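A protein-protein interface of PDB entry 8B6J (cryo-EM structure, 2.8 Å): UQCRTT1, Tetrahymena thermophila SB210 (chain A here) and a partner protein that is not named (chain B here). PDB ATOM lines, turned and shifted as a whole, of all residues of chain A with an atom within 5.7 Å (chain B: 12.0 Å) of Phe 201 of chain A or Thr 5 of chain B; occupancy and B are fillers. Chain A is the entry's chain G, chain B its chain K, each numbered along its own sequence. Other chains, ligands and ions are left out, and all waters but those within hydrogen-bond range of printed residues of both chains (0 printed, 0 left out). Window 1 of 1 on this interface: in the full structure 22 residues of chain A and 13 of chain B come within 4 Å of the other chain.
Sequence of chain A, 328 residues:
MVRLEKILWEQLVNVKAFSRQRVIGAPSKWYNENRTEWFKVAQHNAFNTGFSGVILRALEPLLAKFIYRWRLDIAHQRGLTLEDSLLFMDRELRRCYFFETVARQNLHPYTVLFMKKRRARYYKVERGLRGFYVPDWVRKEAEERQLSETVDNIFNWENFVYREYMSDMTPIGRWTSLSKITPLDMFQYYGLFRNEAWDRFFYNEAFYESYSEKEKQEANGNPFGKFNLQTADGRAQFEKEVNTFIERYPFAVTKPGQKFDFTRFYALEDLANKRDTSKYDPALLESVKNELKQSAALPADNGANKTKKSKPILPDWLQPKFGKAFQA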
ATOM      1  N   LEU A   4      12.919  12.521   6.819  1.00  0.00           N
ATOM      2  CA  LEU A   4      13.042  11.340   7.664  1.00  0.00           C
ATOM      3  C   LEU A   4      13.363  10.108   6.829  1.00  0.00           C
ATOM      4  O   LEU A   4      14.219   9.300   7.207  1.00  0.00           O
ATOM      5  CB  LEU A   4      11.765  11.129   8.475  1.00  0.00           C
ATOM      6  CG  LEU A   4      11.418  12.216   9.498  1.00  0.00           C
ATOM      7  CD1 LEU A   4      10.297  11.744  10.409  1.00  0.00           C
ATOM      8  CD2 LEU A   4      12.632  12.619  10.318  1.00  0.00           C
ATOM      9  N   GLU A   5      12.692   9.946   5.693  1.00  0.00           N
ATOM     10  CA  GLU A   5      13.152   8.975   4.715  1.00  0.00           C
ATOM     11  C   GLU A   5      14.462   9.460   4.107  1.00  0.00           C
ATOM     12  O   GLU A   5      14.710  10.663   3.992  1.00  0.00           O
ATOM     13  CB  GLU A   5      12.097   8.751   3.626  1.00  0.00           C
ATOM     14  CG  GLU A   5      11.939   9.879   2.607  1.00  0.00           C
ATOM     15  CD  GLU A   5      11.303  11.122   3.191  1.00  0.00           C
ATOM     16  OE1 GLU A   5      10.989  11.119   4.398  1.00  0.00           O
ATOM     17  OE2 GLU A   5      11.113  12.102   2.442  1.00  0.00           O
ATOM     18  N   GLU A  10      17.497   4.691   7.535  1.00  0.00           N
ATOM     19  CA  GLU A  10      16.664   4.243   6.424  1.00  0.00           C
ATOM     20  C   GLU A  10      17.517   3.699   5.286  1.00  0.00           C
ATOM     21  O   GLU A  10      17.179   2.676   4.679  1.00  0.00           O
ATOM     22  CB  GLU A  10      15.792   5.398   5.934  1.00  0.00           C
ATOM     23  CG  GLU A  10      14.687   4.992   4.975  1.00  0.00           C
ATOM     24  CD  GLU A  10      13.525   4.320   5.678  1.00  0.00           C
ATOM     25  OE1 GLU A  10      13.575   4.186   6.917  1.00  0.00           O
ATOM     26  OE2 GLU A  10      12.559   3.928   4.989  1.00  0.00           O
ATOM     27  N   ARG A  22      10.696   0.338   1.847  1.00  0.00           N
ATOM     28  CA  ARG A  22       9.403   1.008   1.824  1.00  0.00           C
ATOM     29  C   ARG A  22       8.729   0.774   0.479  1.00  0.00           C
ATOM     30  O   ARG A  22       9.323   1.024  -0.574  1.00  0.00           O
ATOM     31  CB  ARG A  22       9.570   2.506   2.074  1.00  0.00           C
ATOM     32  CG  ARG A  22      10.230   2.858   3.397  1.00  0.00           C
ATOM     33  CD  ARG A  22       9.439   2.320   4.574  1.00  0.00           C
ATOM     34  NE  ARG A  22       9.913   2.850   5.848  1.00  0.00           N
ATOM     35  CZ  ARG A  22       9.447   3.948   6.428  1.00  0.00           C
ATOM     36  NH1 ARG A  22       8.501   4.681   5.864  1.00  0.00           N
ATOM     37  NH2 ARG A  22       9.939   4.317   7.606  1.00  0.00           N
ATOM     38  N   TRP A  30      -6.067   6.283   6.999  1.00  0.00           N
ATOM     39  CA  TRP A  30      -5.528   5.938   8.306  1.00  0.00           C
ATOM     40  C   TRP A  30      -6.574   5.153   9.088  1.00  0.00           C
ATOM     41  O   TRP A  30      -7.780   5.322   8.893  1.00  0.00           O
ATOM     42  CB  TRP A  30      -5.133   7.205   9.063  1.00  0.00           C
ATOM     43  CG  TRP A  30      -4.033   7.017  10.056  1.00  0.00           C
ATOM     44  CD1 TRP A  30      -4.163   6.858  11.401  1.00  0.00           C
ATOM     45  CD2 TRP A  30      -2.627   6.983   9.781  1.00  0.00           C
ATOM     46  NE1 TRP A  30      -2.926   6.723  11.984  1.00  0.00           N
ATOM     47  CE2 TRP A  30      -1.967   6.796  11.009  1.00  0.00           C
ATOM     48  CE3 TRP A  30      -1.865   7.090   8.615  1.00  0.00           C
ATOM     49  CZ2 TRP A  30      -0.582   6.713  11.104  1.00  0.00           C
ATOM     50  CZ3 TRP A  30      -0.490   7.006   8.712  1.00  0.00           C
ATOM     51  CH2 TRP A  30       0.137   6.820   9.947  1.00  0.00           C
ATOM     52  N   PRO A 171      -4.573  11.522  12.409  1.00  0.00           N
ATOM     53  CA  PRO A 171      -3.834  12.207  13.472  1.00  0.00           C
ATOM     54  C   PRO A 171      -2.586  12.890  12.940  1.00  0.00           C
ATOM     55  O   PRO A 171      -2.001  12.481  11.935  1.00  0.00           O
ATOM     56  CB  PRO A 171      -3.482  11.077  14.444  1.00  0.00           C
ATOM     57  CG  PRO A 171      -3.446   9.863  13.601  1.00  0.00           C
ATOM     58  CD  PRO A 171      -4.496  10.057  12.549  1.00  0.00           C
ATOM     59  N   ALA A 197       3.204   6.143  13.722  1.00  0.00           N
ATOM     60  CA  ALA A 197       3.899   7.305  13.181  1.00  0.00           C
ATOM     61  C   ALA A 197       5.134   6.897  12.388  1.00  0.00           C
ATOM     62  O   ALA A 197       5.420   7.472  11.331  1.00  0.00           O
ATOM     63  CB  ALA A 197       4.284   8.255  14.313  1.00  0.00           C
ATOM     64  N   TRP A 198       5.884   5.912  12.884  1.00  0.00           N
ATOM     65  CA  TRP A 198       7.152   5.532  12.275  1.00  0.00           C
ATOM     66  C   TRP A 198       7.043   4.373  11.295  1.00  0.00           C
ATOM     67  O   TRP A 198       7.910   4.241  10.425  1.00  0.00           O
ATOM     68  CB  TRP A 198       8.167   5.168  13.364  1.00  0.00           C
ATOM     69  CG  TRP A 198       8.570   6.338  14.198  1.00  0.00           C
ATOM     70  CD1 TRP A 198       8.072   6.685  15.418  1.00  0.00           C
ATOM     71  CD2 TRP A 198       9.553   7.326  13.871  1.00  0.00           C
ATOM     72  NE1 TRP A 198       8.685   7.825  15.874  1.00  0.00           N
ATOM     73  CE2 TRP A 198       9.599   8.239  14.941  1.00  0.00           C
ATOM     74  CE3 TRP A 198      10.400   7.525  12.777  1.00  0.00           C
ATOM     75  CZ2 TRP A 198      10.459   9.335  14.949  1.00  0.00           C
ATOM     76  CZ3 TRP A 198      11.252   8.613  12.787  1.00  0.00           C
ATOM     77  CH2 TRP A 198      11.275   9.503  13.866  1.00  0.00           C
ATOM     78  N   ASP A 199       6.014   3.531  11.407  1.00  0.00           N
ATOM     79  CA  ASP A 199       5.886   2.411  10.482  1.00  0.00           C
ATOM     80  C   ASP A 199       5.690   2.893   9.051  1.00  0.00           C
ATOM     81  O   ASP A 199       6.299   2.356   8.119  1.00  0.00           O
ATOM     82  CB  ASP A 199       4.726   1.509  10.902  1.00  0.00           C
ATOM     83  CG  ASP A 199       5.064   0.644  12.099  1.00  0.00           C
ATOM     84  OD1 ASP A 199       6.254   0.311  12.278  1.00  0.00           O
ATOM     85  OD2 ASP A 199       4.138   0.290  12.858  1.00  0.00           O
ATOM     86  N   ARG A 200       4.846   3.904   8.856  1.00  0.00           N
ATOM     87  CA  ARG A 200       4.530   4.420   7.530  1.00  0.00           C
ATOM     88  C   ARG A 200       4.663   5.935   7.540  1.00  0.00           C
ATOM     89  O   ARG A 200       3.953   6.616   8.286  1.00  0.00           O
ATOM     90  CB  ARG A 200       3.120   3.999   7.103  1.00  0.00           C
ATOM     91  CG  ARG A 200       2.978   2.503   6.877  1.00  0.00           C
ATOM     92  CD  ARG A 200       1.525   2.059   6.802  1.00  0.00           C
ATOM     93  NE  ARG A 200       0.814   2.639   5.669  1.00  0.00           N
ATOM     94  CZ  ARG A 200       0.021   3.701   5.732  1.00  0.00           C
ATOM     95  NH1 ARG A 200      -0.184   4.348   6.867  1.00  0.00           N
ATOM     96  NH2 ARG A 200      -0.586   4.122   4.627  1.00  0.00           N
ATOM     97  N   PHE A 201       5.573   6.455   6.718  1.00  0.00           N
ATOM     98  CA  PHE A 201       5.756   7.892   6.566  1.00  0.00           C
ATOM     99  C   PHE A 201       4.807   8.511   5.550  1.00  0.00           C
ATOM    100  O   PHE A 201       4.718   9.741   5.480  1.00  0.00           O
ATOM    101  CB  PHE A 201       7.197   8.207   6.139  1.00  0.00           C
ATOM    102  CG  PHE A 201       8.221   8.035   7.230  1.00  0.00           C
ATOM    103  CD1 PHE A 201       7.907   8.277   8.558  1.00  0.00           C
ATOM    104  CD2 PHE A 201       9.510   7.641   6.920  1.00  0.00           C
ATOM    105  CE1 PHE A 201       8.854   8.122   9.545  1.00  0.00           C
ATOM    106  CE2 PHE A 201      10.459   7.486   7.907  1.00  0.00           C
ATOM    107  CZ  PHE A 201      10.131   7.726   9.219  1.00  0.00           C
ATOM    108  N   PHE A 202       4.100   7.700   4.767  1.00  0.00           N
ATOM    109  CA  PHE A 202       3.223   8.194   3.720  1.00  0.00           C
ATOM    110  C   PHE A 202       1.884   7.481   3.806  1.00  0.00           C
ATOM    111  O   PHE A 202       1.780   6.369   4.329  1.00  0.00           O
ATOM    112  CB  PHE A 202       3.824   7.978   2.322  1.00  0.00           C
ATOM    113  CG  PHE A 202       5.267   8.374   2.211  1.00  0.00           C
ATOM    114  CD1 PHE A 202       6.270   7.495   2.579  1.00  0.00           C
ATOM    115  CD2 PHE A 202       5.621   9.620   1.727  1.00  0.00           C
ATOM    116  CE1 PHE A 202       7.597   7.854   2.476  1.00  0.00           C
ATOM    117  CE2 PHE A 202       6.947   9.983   1.620  1.00  0.00           C
ATOM    118  CZ  PHE A 202       7.935   9.099   1.995  1.00  0.00           C
ATOM    119  N   TYR A 203       0.851   8.139   3.282  1.00  0.00           N
ATOM    120  CA  TYR A 203      -0.457   7.516   3.161  1.00  0.00           C
ATOM    121  C   TYR A 203      -0.553   6.599   1.953  1.00  0.00           C
ATOM    122  O   TYR A 203      -1.567   5.913   1.793  1.00  0.00           O
ATOM    123  CB  TYR A 203      -1.541   8.590   3.090  1.00  0.00           C
ATOM    124  CG  TYR A 203      -1.553   9.482   4.305  1.00  0.00           C
ATOM    125  CD1 TYR A 203      -1.990   9.005   5.531  1.00  0.00           C
ATOM    126  CD2 TYR A 203      -1.120  10.796   4.231  1.00  0.00           C
ATOM    127  CE1 TYR A 203      -1.999   9.809   6.646  1.00  0.00           C
ATOM    128  CE2 TYR A 203      -1.127  11.609   5.343  1.00  0.00           C
ATOM    129  CZ  TYR A 203      -1.565  11.109   6.548  1.00  0.00           C
ATOM    130  OH  TYR A 203      -1.574  11.910   7.662  1.00  0.00           O
ATOM    131  N   GLU A 205       2.032   4.309   1.417  1.00  0.00           N
ATOM    132  CA  GLU A 205       2.771   3.105   1.764  1.00  0.00           C
ATOM    133  C   GLU A 205       1.823   1.947   2.039  1.00  0.00           C
ATOM    134  O   GLU A 205       0.797   2.104   2.706  1.00  0.00           O
ATOM    135  CB  GLU A 205       3.654   3.353   2.985  1.00  0.00           C
ATOM    136  CG  GLU A 205       4.910   4.147   2.686  1.00  0.00           C
ATOM    137  CD  GLU A 205       5.943   4.042   3.787  1.00  0.00           C
ATOM    138  OE1 GLU A 205       5.729   3.259   4.734  1.00  0.00           O
ATOM    139  OE2 GLU A 205       6.975   4.740   3.705  1.00  0.00           O
ATOM    140  N   MET B   1       2.473  10.234  -6.481  1.00  0.00           N
ATOM    141  CA  MET B   1       2.350  11.535  -5.766  1.00  0.00           C
ATOM    142  C   MET B   1       2.951  11.439  -4.368  1.00  0.00           C
ATOM    143  O   MET B   1       2.987  10.368  -3.766  1.00  0.00           O
ATOM    144  CB  MET B   1       0.886  11.963  -5.688  1.00  0.00           C
ATOM    145  CG  MET B   1      -0.015  10.954  -5.004  1.00  0.00           C
ATOM    146  SD  MET B   1      -1.760  11.341  -5.201  1.00  0.00           S
ATOM    147  CE  MET B   1      -1.964  11.108  -6.963  1.00  0.00           C
ATOM    148  N   TYR B   2       3.421  12.575  -3.861  1.00  0.00           N
ATOM    149  CA  TYR B   2       4.113  12.642  -2.580  1.00  0.00           C
ATOM    150  C   TYR B   2       3.094  12.979  -1.496  1.00  0.00           C
ATOM    151  O   TYR B   2       2.612  14.113  -1.424  1.00  0.00           O
ATOM    152  CB  TYR B   2       5.226  13.683  -2.648  1.00  0.00           C
ATOM    153  CG  TYR B   2       6.232  13.626  -1.525  1.00  0.00           C
ATOM    154  CD1 TYR B   2       7.159  12.598  -1.450  1.00  0.00           C
ATOM    155  CD2 TYR B   2       6.276  14.619  -0.559  1.00  0.00           C
ATOM    156  CE1 TYR B   2       8.087  12.550  -0.432  1.00  0.00           C
ATOM    157  CE2 TYR B   2       7.198  14.578   0.463  1.00  0.00           C
ATOM    158  CZ  TYR B   2       8.102  13.543   0.521  1.00  0.00           C
ATOM    159  OH  TYR B   2       9.025  13.500   1.538  1.00  0.00           O
ATOM    160  N   LEU B   3       2.777  12.003  -0.648  1.00  0.00           N
ATOM    161  CA  LEU B   3       1.734  12.138   0.370  1.00  0.00           C
ATOM    162  C   LEU B   3       2.309  11.769   1.731  1.00  0.00           C
ATOM    163  O   LEU B   3       1.921  10.762   2.335  1.00  0.00           O
ATOM    164  CB  LEU B   3       0.526  11.264   0.033  1.00  0.00           C
ATOM    165  CG  LEU B   3      -0.354  11.749  -1.119  1.00  0.00           C
ATOM    166  CD1 LEU B   3      -1.348  10.679  -1.525  1.00  0.00           C
ATOM    167  CD2 LEU B   3      -1.085  13.023  -0.733  1.00  0.00           C
ATOM    168  N   PRO B   4       3.234  12.572   2.246  1.00  0.00           N
ATOM    169  CA  PRO B   4       3.831  12.267   3.547  1.00  0.00           C
ATOM    170  C   PRO B   4       2.831  12.424   4.678  1.00  0.00           C
ATOM    171  O   PRO B   4       1.906  13.238   4.620  1.00  0.00           O
ATOM    172  CB  PRO B   4       4.965  13.291   3.661  1.00  0.00           C
ATOM    173  CG  PRO B   4       4.515  14.433   2.832  1.00  0.00           C
ATOM    174  CD  PRO B   4       3.737  13.838   1.692  1.00  0.00           C
ATOM    175  N   THR B   5       3.027  11.623   5.721  1.00  0.00           N
ATOM    176  CA  THR B   5       2.192  11.724   6.907  1.00  0.00           C
ATOM    177  C   THR B   5       2.486  13.021   7.648  1.00  0.00           C
ATOM    178  O   THR B   5       3.614  13.518   7.654  1.00  0.00           O
ATOM    179  CB  THR B   5       2.427  10.528   7.828  1.00  0.00           C
ATOM    180  OG1 THR B   5       2.426   9.321   7.057  1.00  0.00           O
ATOM    181  CG2 THR B   5       1.336  10.444   8.879  1.00  0.00           C
ATOM    182  N   PHE B   6       1.450  13.576   8.278  1.00  0.00           N
ATOM    183  CA  PHE B   6       1.626  14.818   9.020  1.00  0.00           C
ATOM    184  C   PHE B   6       2.517  14.632  10.240  1.00  0.00           C
ATOM    185  O   PHE B   6       3.115  15.608  10.710  1.00  0.00           O
ATOM    186  CB  PHE B   6       0.263  15.377   9.421  1.00  0.00           C
ATOM    187  CG  PHE B   6      -0.636  15.649   8.250  1.00  0.00           C
ATOM    188  CD1 PHE B   6      -0.365  16.691   7.382  1.00  0.00           C
ATOM    189  CD2 PHE B   6      -1.741  14.857   8.008  1.00  0.00           C
ATOM    190  CE1 PHE B   6      -1.182  16.937   6.301  1.00  0.00           C
ATOM    191  CE2 PHE B   6      -2.560  15.099   6.927  1.00  0.00           C
ATOM    192  CZ  PHE B   6      -2.280  16.139   6.074  1.00  0.00           C
ATOM    193  N   TYR B   7       2.633  13.405  10.751  1.00  0.00           N
ATOM    194  CA  TYR B   7       3.652  13.118  11.755  1.00  0.00           C
ATOM    195  C   TYR B   7       5.029  13.521  11.248  1.00  0.00           C
ATOM    196  O   TYR B   7       5.787  14.207  11.940  1.00  0.00           O
ATOM    197  CB  TYR B   7       3.647  11.630  12.106  1.00  0.00           C
ATOM    198  CG  TYR B   7       2.464  11.158  12.916  1.00  0.00           C
ATOM    199  CD1 TYR B   7       2.258  11.612  14.209  1.00  0.00           C
ATOM    200  CD2 TYR B   7       1.574  10.231  12.399  1.00  0.00           C
ATOM    201  CE1 TYR B   7       1.187  11.173  14.955  1.00  0.00           C
ATOM    202  CE2 TYR B   7       0.500   9.785  13.138  1.00  0.00           C
ATOM    203  CZ  TYR B   7       0.312  10.259  14.415  1.00  0.00           C
ATOM    204  OH  TYR B   7      -0.756   9.815  15.155  1.00  0.00           O
ATOM    205  N   LYS B   8       5.368  13.090  10.030  1.00  0.00           N
ATOM    206  CA  LYS B   8       6.687  13.384   9.484  1.00  0.00           C
ATOM    207  C   LYS B   8       6.875  14.877   9.259  1.00  0.00           C
ATOM    208  O   LYS B   8       7.958  15.414   9.514  1.00  0.00           O
ATOM    209  CB  LYS B   8       6.899  12.618   8.181  1.00  0.00           C
ATOM    210  CG  LYS B   8       8.271  12.841   7.574  1.00  0.00           C
ATOM    211  CD  LYS B   8       8.522  11.935   6.392  1.00  0.00           C
ATOM    212  CE  LYS B   8       7.645  12.308   5.221  1.00  0.00           C
ATOM    213  NZ  LYS B   8       8.031  11.563   3.999  1.00  0.00           N
ATOM    214  N   LEU B   9       5.845  15.563   8.758  1.00  0.00           N
ATOM    215  CA  LEU B   9       5.964  17.002   8.551  1.00  0.00           C
ATOM    216  C   LEU B   9       6.213  17.718   9.870  1.00  0.00           C
ATOM    217  O   LEU B   9       7.079  18.599   9.955  1.00  0.00           O
ATOM    218  CB  LEU B   9       4.701  17.542   7.881  1.00  0.00           C
ATOM    219  CG  LEU B   9       4.290  16.866   6.573  1.00  0.00           C
ATOM    220  CD1 LEU B   9       3.079  17.563   5.978  1.00  0.00           C
ATOM    221  CD2 LEU B   9       5.439  16.847   5.580  1.00  0.00           C
ATOM    222  N   PHE B  10       5.468  17.349  10.913  1.00  0.00           N
ATOM    223  CA  PHE B  10       5.682  17.953  12.222  1.00  0.00           C
ATOM    224  C   PHE B  10       7.089  17.673  12.729  1.00  0.00           C
ATOM    225  O   PHE B  10       7.766  18.572  13.243  1.00  0.00           O
ATOM    226  CB  PHE B  10       4.632  17.425  13.200  1.00  0.00           C
ATOM    227  CG  PHE B  10       4.667  18.078  14.548  1.00  0.00           C
ATOM    228  CD1 PHE B  10       4.108  19.327  14.743  1.00  0.00           C
ATOM    229  CD2 PHE B  10       5.240  17.432  15.628  1.00  0.00           C
ATOM    230  CE1 PHE B  10       4.132  19.923  15.986  1.00  0.00           C
ATOM    231  CE2 PHE B  10       5.266  18.025  16.870  1.00  0.00           C
ATOM    232  CZ  PHE B  10       4.713  19.269  17.049  1.00  0.00           C
ATOM    233  N   HIS B  11       7.555  16.431  12.576  1.00  0.00           N
ATOM    234  CA  HIS B  11       8.888  16.073  13.048  1.00  0.00           C
ATOM    235  C   HIS B  11       9.961  16.883  12.332  1.00  0.00           C
ATOM    236  O   HIS B  11      10.892  17.395  12.961  1.00  0.00           O
ATOM    237  CB  HIS B  11       9.129  14.576  12.849  1.00  0.00           C
ATOM    238  CG  HIS B  11       8.231  13.704  13.668  1.00  0.00           C
ATOM    239  ND1 HIS B  11       7.384  14.205  14.632  1.00  0.00           N
ATOM    240  CD2 HIS B  11       8.047  12.363  13.667  1.00  0.00           C
ATOM    241  CE1 HIS B  11       6.717  13.211  15.190  1.00  0.00           C
ATOM    242  NE2 HIS B  11       7.101  12.082  14.622  1.00  0.00           N
ATOM    243  N   GLU B  12       9.850  17.005  11.008  1.00  0.00           N
ATOM    244  CA  GLU B  12      10.857  17.738  10.247  1.00  0.00           C
ATOM    245  C   GLU B  12      10.835  19.224  10.582  1.00  0.00           C
ATOM    246  O   GLU B  12      11.893  19.854  10.719  1.00  0.00           O
ATOM    247  CB  GLU B  12      10.634  17.517   8.752  1.00  0.00           C
ATOM    248  CG  GLU B  12      10.804  16.072   8.315  1.00  0.00           C
ATOM    249  CD  GLU B  12      10.347  15.834   6.890  1.00  0.00           C
ATOM    250  OE1 GLU B  12       9.763  16.757   6.288  1.00  0.00           O
ATOM    251  OE2 GLU B  12      10.573  14.722   6.371  1.00  0.00           O
ATOM    252  N   THR B  13       9.641  19.807  10.718  1.00  0.00           N
ATOM    253  CA  THR B  13       9.555  21.214  11.091  1.00  0.00           C
ATOM    254  C   THR B  13      10.192  21.456  12.453  1.00  0.00           C
ATOM    255  O   THR B  13      10.945  22.421  12.636  1.00  0.00           O
ATOM    256  CB  THR B  13       8.095  21.665  11.097  1.00  0.00           C
ATOM    257  OG1 THR B  13       7.564  21.588   9.770  1.00  0.00           O
ATOM    258  CG2 THR B  13       7.974  23.091  11.611  1.00  0.00           C
ATOM    259  N   ASN B  14       9.906  20.585  13.423  1.00  0.00           N
ATOM    260  CA  ASN B  14      10.491  20.762  14.744  1.00  0.00           C
ATOM    261  C   ASN B  14      11.991  20.508  14.730  1.00  0.00           C
ATOM    262  O   ASN B  14      12.727  21.138  15.493  1.00  0.00           O
ATOM    263  CB  ASN B  14       9.795  19.852  15.750  1.00  0.00           C
ATOM    264  CG  ASN B  14       8.403  20.330  16.087  1.00  0.00           C
ATOM    265  OD1 ASN B  14       8.205  21.077  17.044  1.00  0.00           O
ATOM    266  ND2 ASN B  14       7.429  19.914  15.293  1.00  0.00           N
ATOM    267  N   ALA B  15      12.467  19.605  13.871  1.00  0.00           N
ATOM    268  CA  ALA B  15      13.907  19.413  13.736  1.00  0.00           C
ATOM    269  C   ALA B  15      14.577  20.678  13.219  1.00  0.00           C
ATOM    270  O   ALA B  15      15.623  21.092  13.732  1.00  0.00           O
ATOM    271  CB  ALA B  15      14.196  18.236  12.806  1.00  0.00           C
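Among the printed residues, merely in contact across the chains: Tyr 203 of chain A with Phe 6 of chain B (3.0 Å), Phe 202 of chain A with Lys 8 of chain B (3.1 Å), Pro 171 of chain A with Tyr 7 of chain B (3.1 Å), Phe 202 of chain A with Leu 3 of chain B (3.2 Å), Phe 201 of chain A with Pro 4 of chain B (3.3 Å), Tyr 203 of chain A with Thr 5 of chain B (3.5 Å), Phe 202 of chain A with Tyr 2 of chain B (3.5 Å), Tyr 203 of chain A with Pro 4 of chain B (3.5 Å), Leu 4 of chain A with Lys 8 of chain B (3.7 Å), Phe 202 of chain A with Pro 4 of chain B (3.7 Å), Ala 197 of chain A with Tyr 7 of chain B (3.7 Å), Trp 30 of chain A with Tyr 7 of chain B (3.8 Å), Trp 30 of chain A with Thr 5 of chain B (3.9 Å), Phe 201 of chain A with Lys 8 of chain B (3.9 Å) and Leu 4 of chain A with His 11 of chain B (3.9 Å).
OE2 of Glu 5 of chain A lies within hydrogen-bond range of OH of Tyr 2 of chain B, at 2.7 Å. O of Leu 3 of chain B is in hydrogen-bond range of N of Tyr 203 of chain A, 3.0 Å away. The side-chain hydroxyl (OG1) of Thr 5 of chain B is in hydrogen-bond range of the backbone carbonyl oxygen (O) of Arg 200 of chain A (3.3 Å). The backbone NH (N) of Thr 5 of chain B sits at hydrogen-bond distance from the backbone carbonyl oxygen (O) of Phe 201 of chain A. N of Phe 202 of chain A is in hydrogen-bond range of OG1 of Thr 5 of chain B. NZ of Lys 8 of chain B lies within salt-bridge range of OE1 of Glu 5 of chain A (3.0 Å). The side-chain carboxylate of Glu 12 of chain B lies within hydrogen-bond range of the backbone NH of Leu 4 of chain A (3.2 Å).
Of chain B, only Lys 8 (3.7 Å), His 11 (3.9 Å) and Glu 12 (3.2 Å) come within 4 Å of Leu 4 of chain A. Glu 5 of chain A touches two residues of chain B. Printed residues of chain B within 4 Å of Ala 197 of chain A: Tyr 7. Of chain B, only Thr 5 comes within 4 Å of Arg 200 of chain A. Of chain B, only Pro 4 (3.3 Å), Thr 5 (2.5 Å) and Lys 8 (3.9 Å) come within 4 Å of Phe 201 of chain A. Of chain B, only Tyr 2 (3.5 Å), Leu 3 (3.2 Å), Pro 4 (3.7 Å), Thr 5 (3.3 Å) and Lys 8 (3.1 Å) come within 4 Å of Phe 202 of chain A. Tyr 203 of chain A touches just these residues of chain B: Leu 3 (3.0 Å), Pro 4 (3.5 Å), Thr 5 (3.5 Å) and Phe 6 (3.0 Å). No residue of chain B comes within 4 Å of Glu 205 of chain A. Met 1 of chain B touches none of the printed residues of chain A. Thr 5 of chain B touches just these residues of chain A: Trp 30 (3.9 Å), Arg 200 (3.3 Å), Phe 201 (2.5 Å), Phe 202 (3.3 Å) and Tyr 203 (3.5 Å). Of the printed residues of chain A, Lys 8 of chain B touches Leu 4 (3.7 Å), Glu 5 (3.0 Å), Phe 201 (3.9 Å) and Phe 202 (3.1 Å). Of the printed residues of chain A, His 11 of chain B touches Leu 4. The nearest residue of chain B that does not touch Phe 201 of chain A is Leu 3 of chain B (4.3 Å). The nearest printed residue of chain A that does not touch Lys 8 of chain B is Ala 197 of chain A (5.8 Å).
Hydrophobic or aromatic side chains of chain B that line the printed part of chain A: Tyr 2, Pro 4, Phe 6, Tyr 7 and His 11. Among the printed residues, 22 pairs touch across the chains. Among the printed residues, Asp or Glu carboxylates within 4 Å of a Lys or Arg side-chain nitrogen of the other chain: Glu 5 of chain A with Lys 8 of chain B.
OH of Tyr 2 of chain B sits at hydrogen-bond distance from NZ of Lys 8 of chain B. The backbone carbonyl oxygen (O) of Tyr 7 of chain B lies close to a ring nitrogen (ND1) of His 11 of chain B (3.1 Å). O of Phe 202 of chain A lies within hydrogen-bond range of NH2 of Arg 200 of chain A, at 3.3 Å. O of Tyr 203 of chain A lies within hydrogen-bond range of NH2 of Arg 200 of chain A, 3.5 Å away. NE of Arg 200 of chain A sits at hydrogen-bond distance from O of Glu 205 of chain A (3.0 Å).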
